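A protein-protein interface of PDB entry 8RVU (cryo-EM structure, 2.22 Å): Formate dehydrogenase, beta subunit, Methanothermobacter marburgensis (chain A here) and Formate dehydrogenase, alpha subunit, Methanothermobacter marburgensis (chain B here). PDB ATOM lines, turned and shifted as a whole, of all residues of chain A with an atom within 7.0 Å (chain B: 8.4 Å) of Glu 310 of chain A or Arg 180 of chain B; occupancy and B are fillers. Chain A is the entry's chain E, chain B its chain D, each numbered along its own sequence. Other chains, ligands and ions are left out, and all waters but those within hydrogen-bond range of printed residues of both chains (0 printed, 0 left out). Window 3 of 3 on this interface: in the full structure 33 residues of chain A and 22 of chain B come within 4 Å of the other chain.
NH2 of Arg 180 of chain B sits at hydrogen-bond distance from O of Ile 281 of chain A, at 3.5 Å. NH1 of Arg 180 of chain B lies within salt-bridge range of OE2 of Glu 310 of chain A (3.7 Å).
The side-chain amino group (NZ) of Lys 311 of chain A is in salt-bridge range of the side-chain carboxylate (OE2) of Glu 307 of chain A. NZ of Lys 311 of chain A is in salt-bridge range of OD2 of Asp 309 of chain A (3.0 Å). OG1 of Thr 151 of chain B lies close to OD1 of Asp 148 of chain B, at 3.2 Å. The side-chain carboxylate of Asp 148 of chain B sits at hydrogen-bond distance from the backbone NH of Arg 180 of chain B (3.4 Å). ND2 of Asn 184 of chain B lies within hydrogen-bond range of O of Arg 180 of chain B, at 3.0 Å.
Among the printed residues, merely in contact across the chains: Lys 278 of chain A with Asn 184 of chain B (3.6 Å), Arg 279 of chain A with Phe 161 of chain B (3.6 Å), Glu 310 of chain A with Thr 151 of chain B (3.4 Å) and Lys 311 of chain A with Arg 180 of chain B (3.7 Å).
Of the printed residues of chain B, Ile 281 of chain A touches Arg 180. Glu 310 of chain A touches just these residues of chain B: Thr 151 (3.4 Å) and Arg 180 (3.5 Å). Of the printed residues of chain A, Thr 151 of chain B touches Glu 310. Arg 176 of chain B touches none of the printed residues of chain A. Printed residues of chain A within 4 Å of Arg 180 of chain B: Ile 281, Glu 310 and Lys 311. The nearest residue of chain A that does not touch Arg 180 of chain B is Asp 309 of chain A (4.5 Å). The nearest printed residue of chain B that does not touch Lys 311 of chain A is Glu 178 of chain B (5.2 Å).
Of the 26 printed residues of chain B, 4 touch a printed residue of chain A. Printed residues of chain B that touch a printed residue of chain A: Thr 151, Phe 161, Arg 180 and Asn 184. Hydrophobic or aromatic side chains of chain B within 4 Å of the printed part of chain A: Phe 161. Hydrophobic or aromatic side chains of chain A within 4 Å of the printed part of chain B: Ile 281. Among the printed residues, Asp or Glu carboxylates within 4 Å of a Lys or Arg side-chain nitrogen of the other chain: Glu 310 of chain A with Arg 180 of chain B (3.7 Å).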
ATOM      1  N   LYS A 278      26.564  23.442  39.768  1.00  0.00           N
ATOM      2  CA  LYS A 278      26.902  23.246  38.364  1.00  0.00           C
ATOM      3  C   LYS A 278      26.645  24.496  37.530  1.00  0.00           C
ATOM      4  O   LYS A 278      27.192  24.616  36.429  1.00  0.00           O
ATOM      5  CB  LYS A 278      26.101  22.069  37.806  1.00  0.00           C
ATOM      6  CG  LYS A 278      26.757  21.368  36.620  1.00  0.00           C
ATOM      7  CD  LYS A 278      25.892  20.257  36.007  1.00  0.00           C
ATOM      8  CE  LYS A 278      24.393  20.481  36.182  1.00  0.00           C
ATOM      9  NZ  LYS A 278      23.582  19.501  35.409  1.00  0.00           N
ATOM     10  N   ARG A 279      25.827  25.426  38.030  1.00  0.00           N
ATOM     11  CA  ARG A 279      25.487  26.626  37.274  1.00  0.00           C
ATOM     12  C   ARG A 279      26.550  27.712  37.373  1.00  0.00           C
ATOM     13  O   ARG A 279      26.724  28.484  36.425  1.00  0.00           O
ATOM     14  CB  ARG A 279      24.162  27.204  37.771  1.00  0.00           C
ATOM     15  CG  ARG A 279      22.927  26.553  37.206  1.00  0.00           C
ATOM     16  CD  ARG A 279      21.705  27.393  37.526  1.00  0.00           C
ATOM     17  NE  ARG A 279      20.528  26.584  37.817  1.00  0.00           N
ATOM     18  CZ  ARG A 279      19.498  26.995  38.544  1.00  0.00           C
ATOM     19  NH1 ARG A 279      19.464  28.208  39.074  1.00  0.00           N
ATOM     20  NH2 ARG A 279      18.474  26.171  38.742  1.00  0.00           N
ATOM     21  N   CYS A 280      27.258  27.787  38.500  1.00  0.00           N
ATOM     22  CA  CYS A 280      28.056  28.966  38.824  1.00  0.00           C
ATOM     23  C   CYS A 280      28.972  29.352  37.671  1.00  0.00           C
ATOM     24  O   CYS A 280      29.674  28.511  37.107  1.00  0.00           O
ATOM     25  CB  CYS A 280      28.877  28.699  40.086  1.00  0.00           C
ATOM     26  SG  CYS A 280      30.002  30.036  40.543  1.00  0.00           S
ATOM     27  N   ILE A 281      28.954  30.639  37.323  1.00  0.00           N
ATOM     28  CA  ILE A 281      29.771  31.169  36.237  1.00  0.00           C
ATOM     29  C   ILE A 281      31.012  31.887  36.755  1.00  0.00           C
ATOM     30  O   ILE A 281      31.722  32.527  35.975  1.00  0.00           O
ATOM     31  CB  ILE A 281      28.945  32.095  35.326  1.00  0.00           C
ATOM     32  CG1 ILE A 281      28.227  33.167  36.149  1.00  0.00           C
ATOM     33  CG2 ILE A 281      27.938  31.289  34.522  1.00  0.00           C
ATOM     34  CD1 ILE A 281      28.064  34.480  35.420  1.00  0.00           C
ATOM     35  N   ASN A 282      31.289  31.799  38.057  1.00  0.00           N
ATOM     36  CA  ASN A 282      32.517  32.347  38.633  1.00  0.00           C
ATOM     37  C   ASN A 282      32.613  33.855  38.411  1.00  0.00           C
ATOM     38  O   ASN A 282      33.685  34.393  38.126  1.00  0.00           O
ATOM     39  CB  ASN A 282      33.743  31.634  38.060  1.00  0.00           C
ATOM     40  CG  ASN A 282      34.921  31.641  39.008  1.00  0.00           C
ATOM     41  OD1 ASN A 282      34.781  31.348  40.194  1.00  0.00           O
ATOM     42  ND2 ASN A 282      36.096  31.970  38.486  1.00  0.00           N
ATOM     43  N   CYS A 283      31.480  34.546  38.541  1.00  0.00           N
ATOM     44  CA  CYS A 283      31.428  35.984  38.312  1.00  0.00           C
ATOM     45  C   CYS A 283      31.784  36.802  39.546  1.00  0.00           C
ATOM     46  O   CYS A 283      32.051  38.001  39.413  1.00  0.00           O
ATOM     47  CB  CYS A 283      30.033  36.379  37.825  1.00  0.00           C
ATOM     48  SG  CYS A 283      28.753  36.306  39.097  1.00  0.00           S
ATOM     49  N   GLU A 307      39.400  29.274  39.431  1.00  0.00           N
ATOM     50  CA  GLU A 307      39.105  28.359  38.335  1.00  0.00           C
ATOM     51  C   GLU A 307      39.317  29.107  37.024  1.00  0.00           C
ATOM     52  O   GLU A 307      38.544  30.007  36.682  1.00  0.00           O
ATOM     53  CB  GLU A 307      37.678  27.829  38.456  1.00  0.00           C
ATOM     54  CG  GLU A 307      37.512  26.396  37.997  1.00  0.00           C
ATOM     55  CD  GLU A 307      37.075  26.300  36.559  1.00  0.00           C
ATOM     56  OE1 GLU A 307      36.032  26.892  36.214  1.00  0.00           O
ATOM     57  OE2 GLU A 307      37.775  25.631  35.773  1.00  0.00           O
ATOM     58  N   SER A 308      40.365  28.737  36.294  1.00  0.00           N
ATOM     59  CA  SER A 308      40.798  29.473  35.114  1.00  0.00           C
ATOM     60  C   SER A 308      40.100  29.032  33.836  1.00  0.00           C
ATOM     61  O   SER A 308      40.305  29.657  32.791  1.00  0.00           O
ATOM     62  CB  SER A 308      42.313  29.334  34.942  1.00  0.00           C
ATOM     63  OG  SER A 308      42.740  28.024  35.269  1.00  0.00           O
ATOM     64  N   ASP A 309      39.290  27.981  33.885  1.00  0.00           N
ATOM     65  CA  ASP A 309      38.561  27.509  32.718  1.00  0.00           C
ATOM     66  C   ASP A 309      37.128  28.027  32.747  1.00  0.00           C
ATOM     67  O   ASP A 309      36.604  28.428  33.788  1.00  0.00           O
ATOM     68  CB  ASP A 309      38.568  25.980  32.655  1.00  0.00           C
ATOM     69  CG  ASP A 309      39.946  25.413  32.374  1.00  0.00           C
ATOM     70  OD1 ASP A 309      40.786  26.142  31.807  1.00  0.00           O
ATOM     71  OD2 ASP A 309      40.187  24.238  32.719  1.00  0.00           O
ATOM     72  N   GLU A 310      36.496  28.013  31.575  1.00  0.00           N
ATOM     73  CA  GLU A 310      35.134  28.524  31.422  1.00  0.00           C
ATOM     74  C   GLU A 310      34.133  27.411  31.739  1.00  0.00           C
ATOM     75  O   GLU A 310      33.377  26.937  30.889  1.00  0.00           O
ATOM     76  CB  GLU A 310      34.931  29.084  30.019  1.00  0.00           C
ATOM     77  CG  GLU A 310      35.933  30.160  29.625  1.00  0.00           C
ATOM     78  CD  GLU A 310      35.504  31.549  30.057  1.00  0.00           C
ATOM     79  OE1 GLU A 310      35.821  31.944  31.199  1.00  0.00           O
ATOM     80  OE2 GLU A 310      34.849  32.248  29.255  1.00  0.00           O
ATOM     81  N   LYS A 311      34.146  26.997  33.004  1.00  0.00           N
ATOM     82  CA  LYS A 311      33.203  26.007  33.501  1.00  0.00           C
ATOM     83  C   LYS A 311      32.891  26.322  34.956  1.00  0.00           C
ATOM     84  O   LYS A 311      33.523  27.177  35.579  1.00  0.00           O
ATOM     85  CB  LYS A 311      33.744  24.581  33.360  1.00  0.00           C
ATOM     86  CG  LYS A 311      35.158  24.385  33.875  1.00  0.00           C
ATOM     87  CD  LYS A 311      35.326  22.996  34.476  1.00  0.00           C
ATOM     88  CE  LYS A 311      36.775  22.674  34.818  1.00  0.00           C
ATOM     89  NZ  LYS A 311      37.714  22.898  33.684  1.00  0.00           N
ATOM     90  N   ALA A 312      31.899  25.622  35.492  1.00  0.00           N
ATOM     91  CA  ALA A 312      31.488  25.860  36.866  1.00  0.00           C
ATOM     92  C   ALA A 312      32.635  25.520  37.813  1.00  0.00           C
ATOM     93  O   ALA A 312      33.237  24.444  37.687  1.00  0.00           O
ATOM     94  CB  ALA A 312      30.254  25.027  37.210  1.00  0.00           C
ATOM     95  N   PRO A 313      32.970  26.391  38.761  1.00  0.00           N
ATOM     96  CA  PRO A 313      34.068  26.083  39.681  1.00  0.00           C
ATOM     97  C   PRO A 313      33.684  24.999  40.672  1.00  0.00           C
ATOM     98  O   PRO A 313      32.509  24.757  40.955  1.00  0.00           O
ATOM     99  CB  PRO A 313      34.321  27.417  40.391  1.00  0.00           C
ATOM    100  CG  PRO A 313      33.014  28.116  40.338  1.00  0.00           C
ATOM    101  CD  PRO A 313      32.389  27.718  39.030  1.00  0.00           C
ATOM    102  N   VAL B 145      20.108  25.979  20.696  1.00  0.00           N
ATOM    103  CA  VAL B 145      21.141  26.959  21.007  1.00  0.00           C
ATOM    104  C   VAL B 145      22.357  26.652  20.148  1.00  0.00           C
ATOM    105  O   VAL B 145      22.918  25.554  20.225  1.00  0.00           O
ATOM    106  CB  VAL B 145      21.506  26.945  22.500  1.00  0.00           C
ATOM    107  CG1 VAL B 145      22.750  27.783  22.752  1.00  0.00           C
ATOM    108  CG2 VAL B 145      20.338  27.448  23.336  1.00  0.00           C
ATOM    109  N   GLY B 147      26.126  27.902  19.509  1.00  0.00           N
ATOM    110  CA  GLY B 147      27.149  28.658  20.198  1.00  0.00           C
ATOM    111  C   GLY B 147      26.928  28.693  21.701  1.00  0.00           C
ATOM    112  O   GLY B 147      25.837  28.438  22.211  1.00  0.00           O
ATOM    113  N   ASP B 148      27.998  29.023  22.421  1.00  0.00           N
ATOM    114  CA  ASP B 148      27.963  29.098  23.881  1.00  0.00           C
ATOM    115  C   ASP B 148      27.235  30.377  24.276  1.00  0.00           C
ATOM    116  O   ASP B 148      27.832  31.445  24.420  1.00  0.00           O
ATOM    117  CB  ASP B 148      29.371  29.055  24.458  1.00  0.00           C
ATOM    118  CG  ASP B 148      29.380  28.945  25.969  1.00  0.00           C
ATOM    119  OD1 ASP B 148      28.289  28.953  26.576  1.00  0.00           O
ATOM    120  OD2 ASP B 148      30.480  28.855  26.551  1.00  0.00           O
ATOM    121  N   ALA B 149      25.918  30.263  24.458  1.00  0.00           N
ATOM    122  CA  ALA B 149      25.109  31.438  24.762  1.00  0.00           C
ATOM    123  C   ALA B 149      25.389  31.963  26.164  1.00  0.00           C
ATOM    124  O   ALA B 149      25.364  33.177  26.392  1.00  0.00           O
ATOM    125  CB  ALA B 149      23.627  31.105  24.603  1.00  0.00           C
ATOM    126  N   ILE B 150      25.653  31.069  27.119  1.00  0.00           N
ATOM    127  CA  ILE B 150      25.879  31.502  28.495  1.00  0.00           C
ATOM    128  C   ILE B 150      27.113  32.394  28.572  1.00  0.00           C
ATOM    129  O   ILE B 150      27.089  33.465  29.189  1.00  0.00           O
ATOM    130  CB  ILE B 150      26.007  30.287  29.430  1.00  0.00           C
ATOM    131  CG1 ILE B 150      24.677  29.535  29.518  1.00  0.00           C
ATOM    132  CG2 ILE B 150      26.450  30.728  30.815  1.00  0.00           C
ATOM    133  CD1 ILE B 150      24.821  28.092  29.943  1.00  0.00           C
ATOM    134  N   THR B 151      28.211  31.964  27.948  1.00  0.00           N
ATOM    135  CA  THR B 151      29.428  32.767  27.972  1.00  0.00           C
ATOM    136  C   THR B 151      29.245  34.073  27.206  1.00  0.00           C
ATOM    137  O   THR B 151      29.702  35.130  27.654  1.00  0.00           O
ATOM    138  CB  THR B 151      30.595  31.967  27.395  1.00  0.00           C
ATOM    139  OG1 THR B 151      30.631  30.669  28.001  1.00  0.00           O
ATOM    140  CG2 THR B 151      31.913  32.680  27.654  1.00  0.00           C
ATOM    141  N   CYS B 152      28.580  34.019  26.051  1.00  0.00           N
ATOM    142  CA  CYS B 152      28.376  35.226  25.256  1.00  0.00           C
ATOM    143  C   CYS B 152      27.523  36.242  26.008  1.00  0.00           C
ATOM    144  O   CYS B 152      27.819  37.442  26.007  1.00  0.00           O
ATOM    145  CB  CYS B 152      27.734  34.866  23.916  1.00  0.00           C
ATOM    146  SG  CYS B 152      28.851  34.040  22.759  1.00  0.00           S
ATOM    147  N   PRO B 154      25.782  36.018  29.758  1.00  0.00           N
ATOM    148  CA  PRO B 154      25.391  35.259  30.957  1.00  0.00           C
ATOM    149  C   PRO B 154      23.956  35.489  31.397  1.00  0.00           C
ATOM    150  O   PRO B 154      23.300  34.543  31.855  1.00  0.00           O
ATOM    151  CB  PRO B 154      26.385  35.756  32.011  1.00  0.00           C
ATOM    152  CG  PRO B 154      27.604  36.084  31.233  1.00  0.00           C
ATOM    153  CD  PRO B 154      27.124  36.611  29.902  1.00  0.00           C
ATOM    154  N   GLY B 157      21.739  33.363  29.293  1.00  0.00           N
ATOM    155  CA  GLY B 157      21.853  31.998  29.773  1.00  0.00           C
ATOM    156  C   GLY B 157      21.079  31.776  31.055  1.00  0.00           C
ATOM    157  O   GLY B 157      20.602  30.670  31.315  1.00  0.00           O
ATOM    158  N   PHE B 161      18.377  28.858  31.585  1.00  0.00           N
ATOM    159  CA  PHE B 161      18.244  27.999  32.758  1.00  0.00           C
ATOM    160  C   PHE B 161      16.821  28.031  33.301  1.00  0.00           C
ATOM    161  O   PHE B 161      16.266  26.991  33.681  1.00  0.00           O
ATOM    162  CB  PHE B 161      19.232  28.431  33.842  1.00  0.00           C
ATOM    163  CG  PHE B 161      20.603  27.843  33.683  1.00  0.00           C
ATOM    164  CD1 PHE B 161      20.819  26.491  33.885  1.00  0.00           C
ATOM    165  CD2 PHE B 161      21.679  28.647  33.346  1.00  0.00           C
ATOM    166  CE1 PHE B 161      22.080  25.951  33.740  1.00  0.00           C
ATOM    167  CE2 PHE B 161      22.940  28.110  33.204  1.00  0.00           C
ATOM    168  CZ  PHE B 161      23.141  26.762  33.402  1.00  0.00           C
ATOM    169  N   MET B 164      14.851  25.802  31.229  1.00  0.00           N
ATOM    170  CA  MET B 164      15.130  24.411  31.570  1.00  0.00           C
ATOM    171  C   MET B 164      14.319  23.986  32.787  1.00  0.00           C
ATOM    172  O   MET B 164      13.725  22.902  32.807  1.00  0.00           O
ATOM    173  CB  MET B 164      16.622  24.230  31.835  1.00  0.00           C
ATOM    174  CG  MET B 164      17.424  23.858  30.611  1.00  0.00           C
ATOM    175  SD  MET B 164      19.164  24.267  30.816  1.00  0.00           S
ATOM    176  CE  MET B 164      19.798  23.798  29.215  1.00  0.00           C
ATOM    177  N   SER B 172      21.937  22.002  22.162  1.00  0.00           N
ATOM    178  CA  SER B 172      22.946  22.955  21.903  1.00  0.00           C
ATOM    179  C   SER B 172      23.839  22.426  20.890  1.00  0.00           C
ATOM    180  O   SER B 172      23.906  21.318  20.751  1.00  0.00           O
ATOM    181  CB  SER B 172      23.634  23.216  23.041  1.00  0.00           C
ATOM    182  OG  SER B 172      24.158  22.123  23.652  1.00  0.00           O
ATOM    183  N   ASP B 174      27.549  23.235  18.791  1.00  0.00           N
ATOM    184  CA  ASP B 174      28.786  24.000  18.710  1.00  0.00           C
ATOM    185  C   ASP B 174      29.868  23.097  18.131  1.00  0.00           C
ATOM    186  O   ASP B 174      29.660  21.898  17.931  1.00  0.00           O
ATOM    187  CB  ASP B 174      29.188  24.548  20.081  1.00  0.00           C
ATOM    188  CG  ASP B 174      30.073  25.774  19.983  1.00  0.00           C
ATOM    189  OD1 ASP B 174      30.937  25.813  19.083  1.00  0.00           O
ATOM    190  OD2 ASP B 174      29.903  26.699  20.804  1.00  0.00           O
ATOM    191  N   ARG B 176      32.619  22.763  19.823  1.00  0.00           N
ATOM    192  CA  ARG B 176      33.295  22.319  21.030  1.00  0.00           C
ATOM    193  C   ARG B 176      32.298  21.567  21.901  1.00  0.00           C
ATOM    194  O   ARG B 176      31.085  21.760  21.795  1.00  0.00           O
ATOM    195  CB  ARG B 176      33.898  23.500  21.802  1.00  0.00           C
ATOM    196  CG  ARG B 176      35.045  24.183  21.072  1.00  0.00           C
ATOM    197  CD  ARG B 176      35.198  25.640  21.483  1.00  0.00           C
ATOM    198  NE  ARG B 176      34.001  26.422  21.188  1.00  0.00           N
ATOM    199  CZ  ARG B 176      33.496  27.365  21.972  1.00  0.00           C
ATOM    200  NH1 ARG B 176      34.071  27.700  23.116  1.00  0.00           N
ATOM    201  NH2 ARG B 176      32.386  27.993  21.596  1.00  0.00           N
ATOM    202  N   ASP B 177      32.824  20.703  22.768  1.00  0.00           N
ATOM    203  CA  ASP B 177      31.998  19.789  23.547  1.00  0.00           C
ATOM    204  C   ASP B 177      32.132  20.013  25.050  1.00  0.00           C
ATOM    205  O   ASP B 177      31.688  19.168  25.833  1.00  0.00           O
ATOM    206  CB  ASP B 177      32.358  18.343  23.194  1.00  0.00           C
ATOM    207  CG  ASP B 177      31.261  17.354  23.559  1.00  0.00           C
ATOM    208  OD1 ASP B 177      30.458  17.643  24.468  1.00  0.00           O
ATOM    209  OD2 ASP B 177      31.205  16.278  22.930  1.00  0.00           O
ATOM    210  N   GLU B 178      32.736  21.125  25.475  1.00  0.00           N
ATOM    211  CA  GLU B 178      32.869  21.401  26.900  1.00  0.00           C
ATOM    212  C   GLU B 178      32.491  22.833  27.266  1.00  0.00           C
ATOM    213  O   GLU B 178      32.808  23.274  28.377  1.00  0.00           O
ATOM    214  CB  GLU B 178      34.302  21.089  27.375  1.00  0.00           C
ATOM    215  CG  GLU B 178      35.340  22.180  27.122  1.00  0.00           C
ATOM    216  CD  GLU B 178      35.784  22.232  25.676  1.00  0.00           C
ATOM    217  OE1 GLU B 178      36.994  22.419  25.433  1.00  0.00           O
ATOM    218  OE2 GLU B 178      34.923  22.082  24.783  1.00  0.00           O
ATOM    219  N   THR B 179      31.823  23.566  26.380  1.00  0.00           N
ATOM    220  CA  THR B 179      31.382  24.909  26.715  1.00  0.00           C
ATOM    221  C   THR B 179      30.301  24.852  27.794  1.00  0.00           C
ATOM    222  O   THR B 179      29.794  23.787  28.153  1.00  0.00           O
ATOM    223  CB  THR B 179      30.858  25.625  25.470  1.00  0.00           C
ATOM    224  OG1 THR B 179      29.693  24.951  24.980  1.00  0.00           O
ATOM    225  CG2 THR B 179      31.920  25.657  24.380  1.00  0.00           C
ATOM    226  N   ARG B 180      29.953  26.028  28.322  1.00  0.00           N
ATOM    227  CA  ARG B 180      28.959  26.085  29.390  1.00  0.00           C
ATOM    228  C   ARG B 180      27.617  25.539  28.921  1.00  0.00           C
ATOM    229  O   ARG B 180      26.963  24.774  29.642  1.00  0.00           O
ATOM    230  CB  ARG B 180      28.807  27.523  29.889  1.00  0.00           C
ATOM    231  CG  ARG B 180      30.025  28.057  30.626  1.00  0.00           C
ATOM    232  CD  ARG B 180      29.680  29.273  31.471  1.00  0.00           C
ATOM    233  NE  ARG B 180      30.660  29.498  32.529  1.00  0.00           N
ATOM    234  CZ  ARG B 180      31.762  30.226  32.396  1.00  0.00           C
ATOM    235  NH1 ARG B 180      32.065  30.823  31.255  1.00  0.00           N
ATOM    236  NH2 ARG B 180      32.581  30.354  33.435  1.00  0.00           N
ATOM    237  N   MET B 181      27.190  25.915  27.714  1.00  0.00           N
ATOM    238  CA  MET B 181      25.949  25.370  27.175  1.00  0.00           C
ATOM    239  C   MET B 181      26.054  23.864  26.985  1.00  0.00           C
ATOM    240  O   MET B 181      25.121  23.121  27.310  1.00  0.00           O
ATOM    241  CB  MET B 181      25.603  26.058  25.854  1.00  0.00           C
ATOM    242  CG  MET B 181      24.823  27.360  26.009  1.00  0.00           C
ATOM    243  SD  MET B 181      23.220  27.193  26.827  1.00  0.00           S
ATOM    244  CE  MET B 181      22.637  25.628  26.183  1.00  0.00           C
ATOM    245  N   ALA B 182      27.192  23.390  26.472  1.00  0.00           N
ATOM    246  CA  ALA B 182      27.377  21.954  26.288  1.00  0.00           C
ATOM    247  C   ALA B 182      27.241  21.213  27.611  1.00  0.00           C
ATOM    248  O   ALA B 182      26.649  20.130  27.667  1.00  0.00           O
ATOM    249  CB  ALA B 182      28.742  21.679  25.659  1.00  0.00           C
ATOM    250  N   VAL B 183      27.788  21.781  28.686  1.00  0.00           N
ATOM    251  CA  VAL B 183      27.710  21.131  29.990  1.00  0.00           C
ATOM    252  C   VAL B 183      26.283  21.163  30.521  1.00  0.00           C
ATOM    253  O   VAL B 183      25.781  20.162  31.048  1.00  0.00           O
ATOM    254  CB  VAL B 183      28.689  21.799  30.973  1.00  0.00           C
ATOM    255  CG1 VAL B 183      28.422  21.324  32.393  1.00  0.00           C
ATOM    256  CG2 VAL B 183      30.124  21.513  30.568  1.00  0.00           C
ATOM    257  N   ASN B 184      25.604  22.303  30.393  1.00  0.00           N
ATOM    258  CA  ASN B 184      24.305  22.498  31.020  1.00  0.00           C
ATOM    259  C   ASN B 184      23.128  22.246  30.087  1.00  0.00           C
ATOM    260  O   ASN B 184      21.979  22.357  30.530  1.00  0.00           O
ATOM    261  CB  ASN B 184      24.201  23.923  31.577  1.00  0.00           C
ATOM    262  CG  ASN B 184      25.085  24.140  32.787  1.00  0.00           C
ATOM    263  OD1 ASN B 184      24.727  23.772  33.905  1.00  0.00           O
ATOM    264  ND2 ASN B 184      26.249  24.739  32.568  1.00  0.00           N
ATOM    265  N   SER B 185      23.371  21.909  28.825  1.00  0.00           N
ATOM    266  CA  SER B 185      22.279  21.693  27.891  1.00  0.00           C
ATOM    267  C   SER B 185      21.614  20.341  28.136  1.00  0.00           C
ATOM    268  O   SER B 185      22.223  19.400  28.652  1.00  0.00           O
ATOM    269  CB  SER B 185      22.776  21.766  26.448  1.00  0.00           C
ATOM    270  OG  SER B 185      23.928  20.965  26.268  1.00  0.00           O
ATOM    271  N   GLY B 186      20.338  20.259  27.757  1.00  0.00           N
ATOM    272  CA  GLY B 186      19.656  18.977  27.791  1.00  0.00           C
ATOM    273  C   GLY B 186      20.296  17.969  26.858  1.00  0.00           C
ATOM    274  O   GLY B 186      20.343  16.773  27.154  1.00  0.00           O
ATOM    275  N   HIS B 188      23.704  18.040  23.807  1.00  0.00           N
ATOM    276  CA  HIS B 188      24.712  18.789  23.074  1.00  0.00           C
ATOM    277  C   HIS B 188      25.223  17.962  21.905  1.00  0.00           C
ATOM    278  O   HIS B 188      25.332  16.736  21.990  1.00  0.00           O
ATOM    279  CB  HIS B 188      25.889  19.188  23.972  1.00  0.00           C
ATOM    280  CG  HIS B 188      26.991  19.887  23.240  1.00  0.00           C
ATOM    281  ND1 HIS B 188      26.906  21.207  22.853  1.00  0.00           N
ATOM    282  CD2 HIS B 188      28.201  19.450  22.820  1.00  0.00           C
ATOM    283  CE1 HIS B 188      28.017  21.552  22.226  1.00  0.00           C
ATOM    284  NE2 HIS B 188      28.819  20.505  22.193  1.00  0.00           N
ATOM    285  N   GLU B 215      29.607  32.921  17.309  1.00  0.00           N
ATOM    286  CA  GLU B 215      30.792  32.072  17.358  1.00  0.00           C
ATOM    287  C   GLU B 215      30.947  31.249  16.086  1.00  0.00           C
ATOM    288  O   GLU B 215      32.074  30.932  15.689  1.00  0.00           O
ATOM    289  CB  GLU B 215      30.720  31.158  18.581  1.00  0.00           C
ATOM    290  CG  GLU B 215      30.598  31.912  19.895  1.00  0.00           C
ATOM    291  CD  GLU B 215      31.406  31.280  21.010  1.00  0.00           C
ATOM    292  OE1 GLU B 215      30.951  30.260  21.567  1.00  0.00           O
ATOM    293  OE2 GLU B 215      32.493  31.805  21.332  1.00  0.00           O
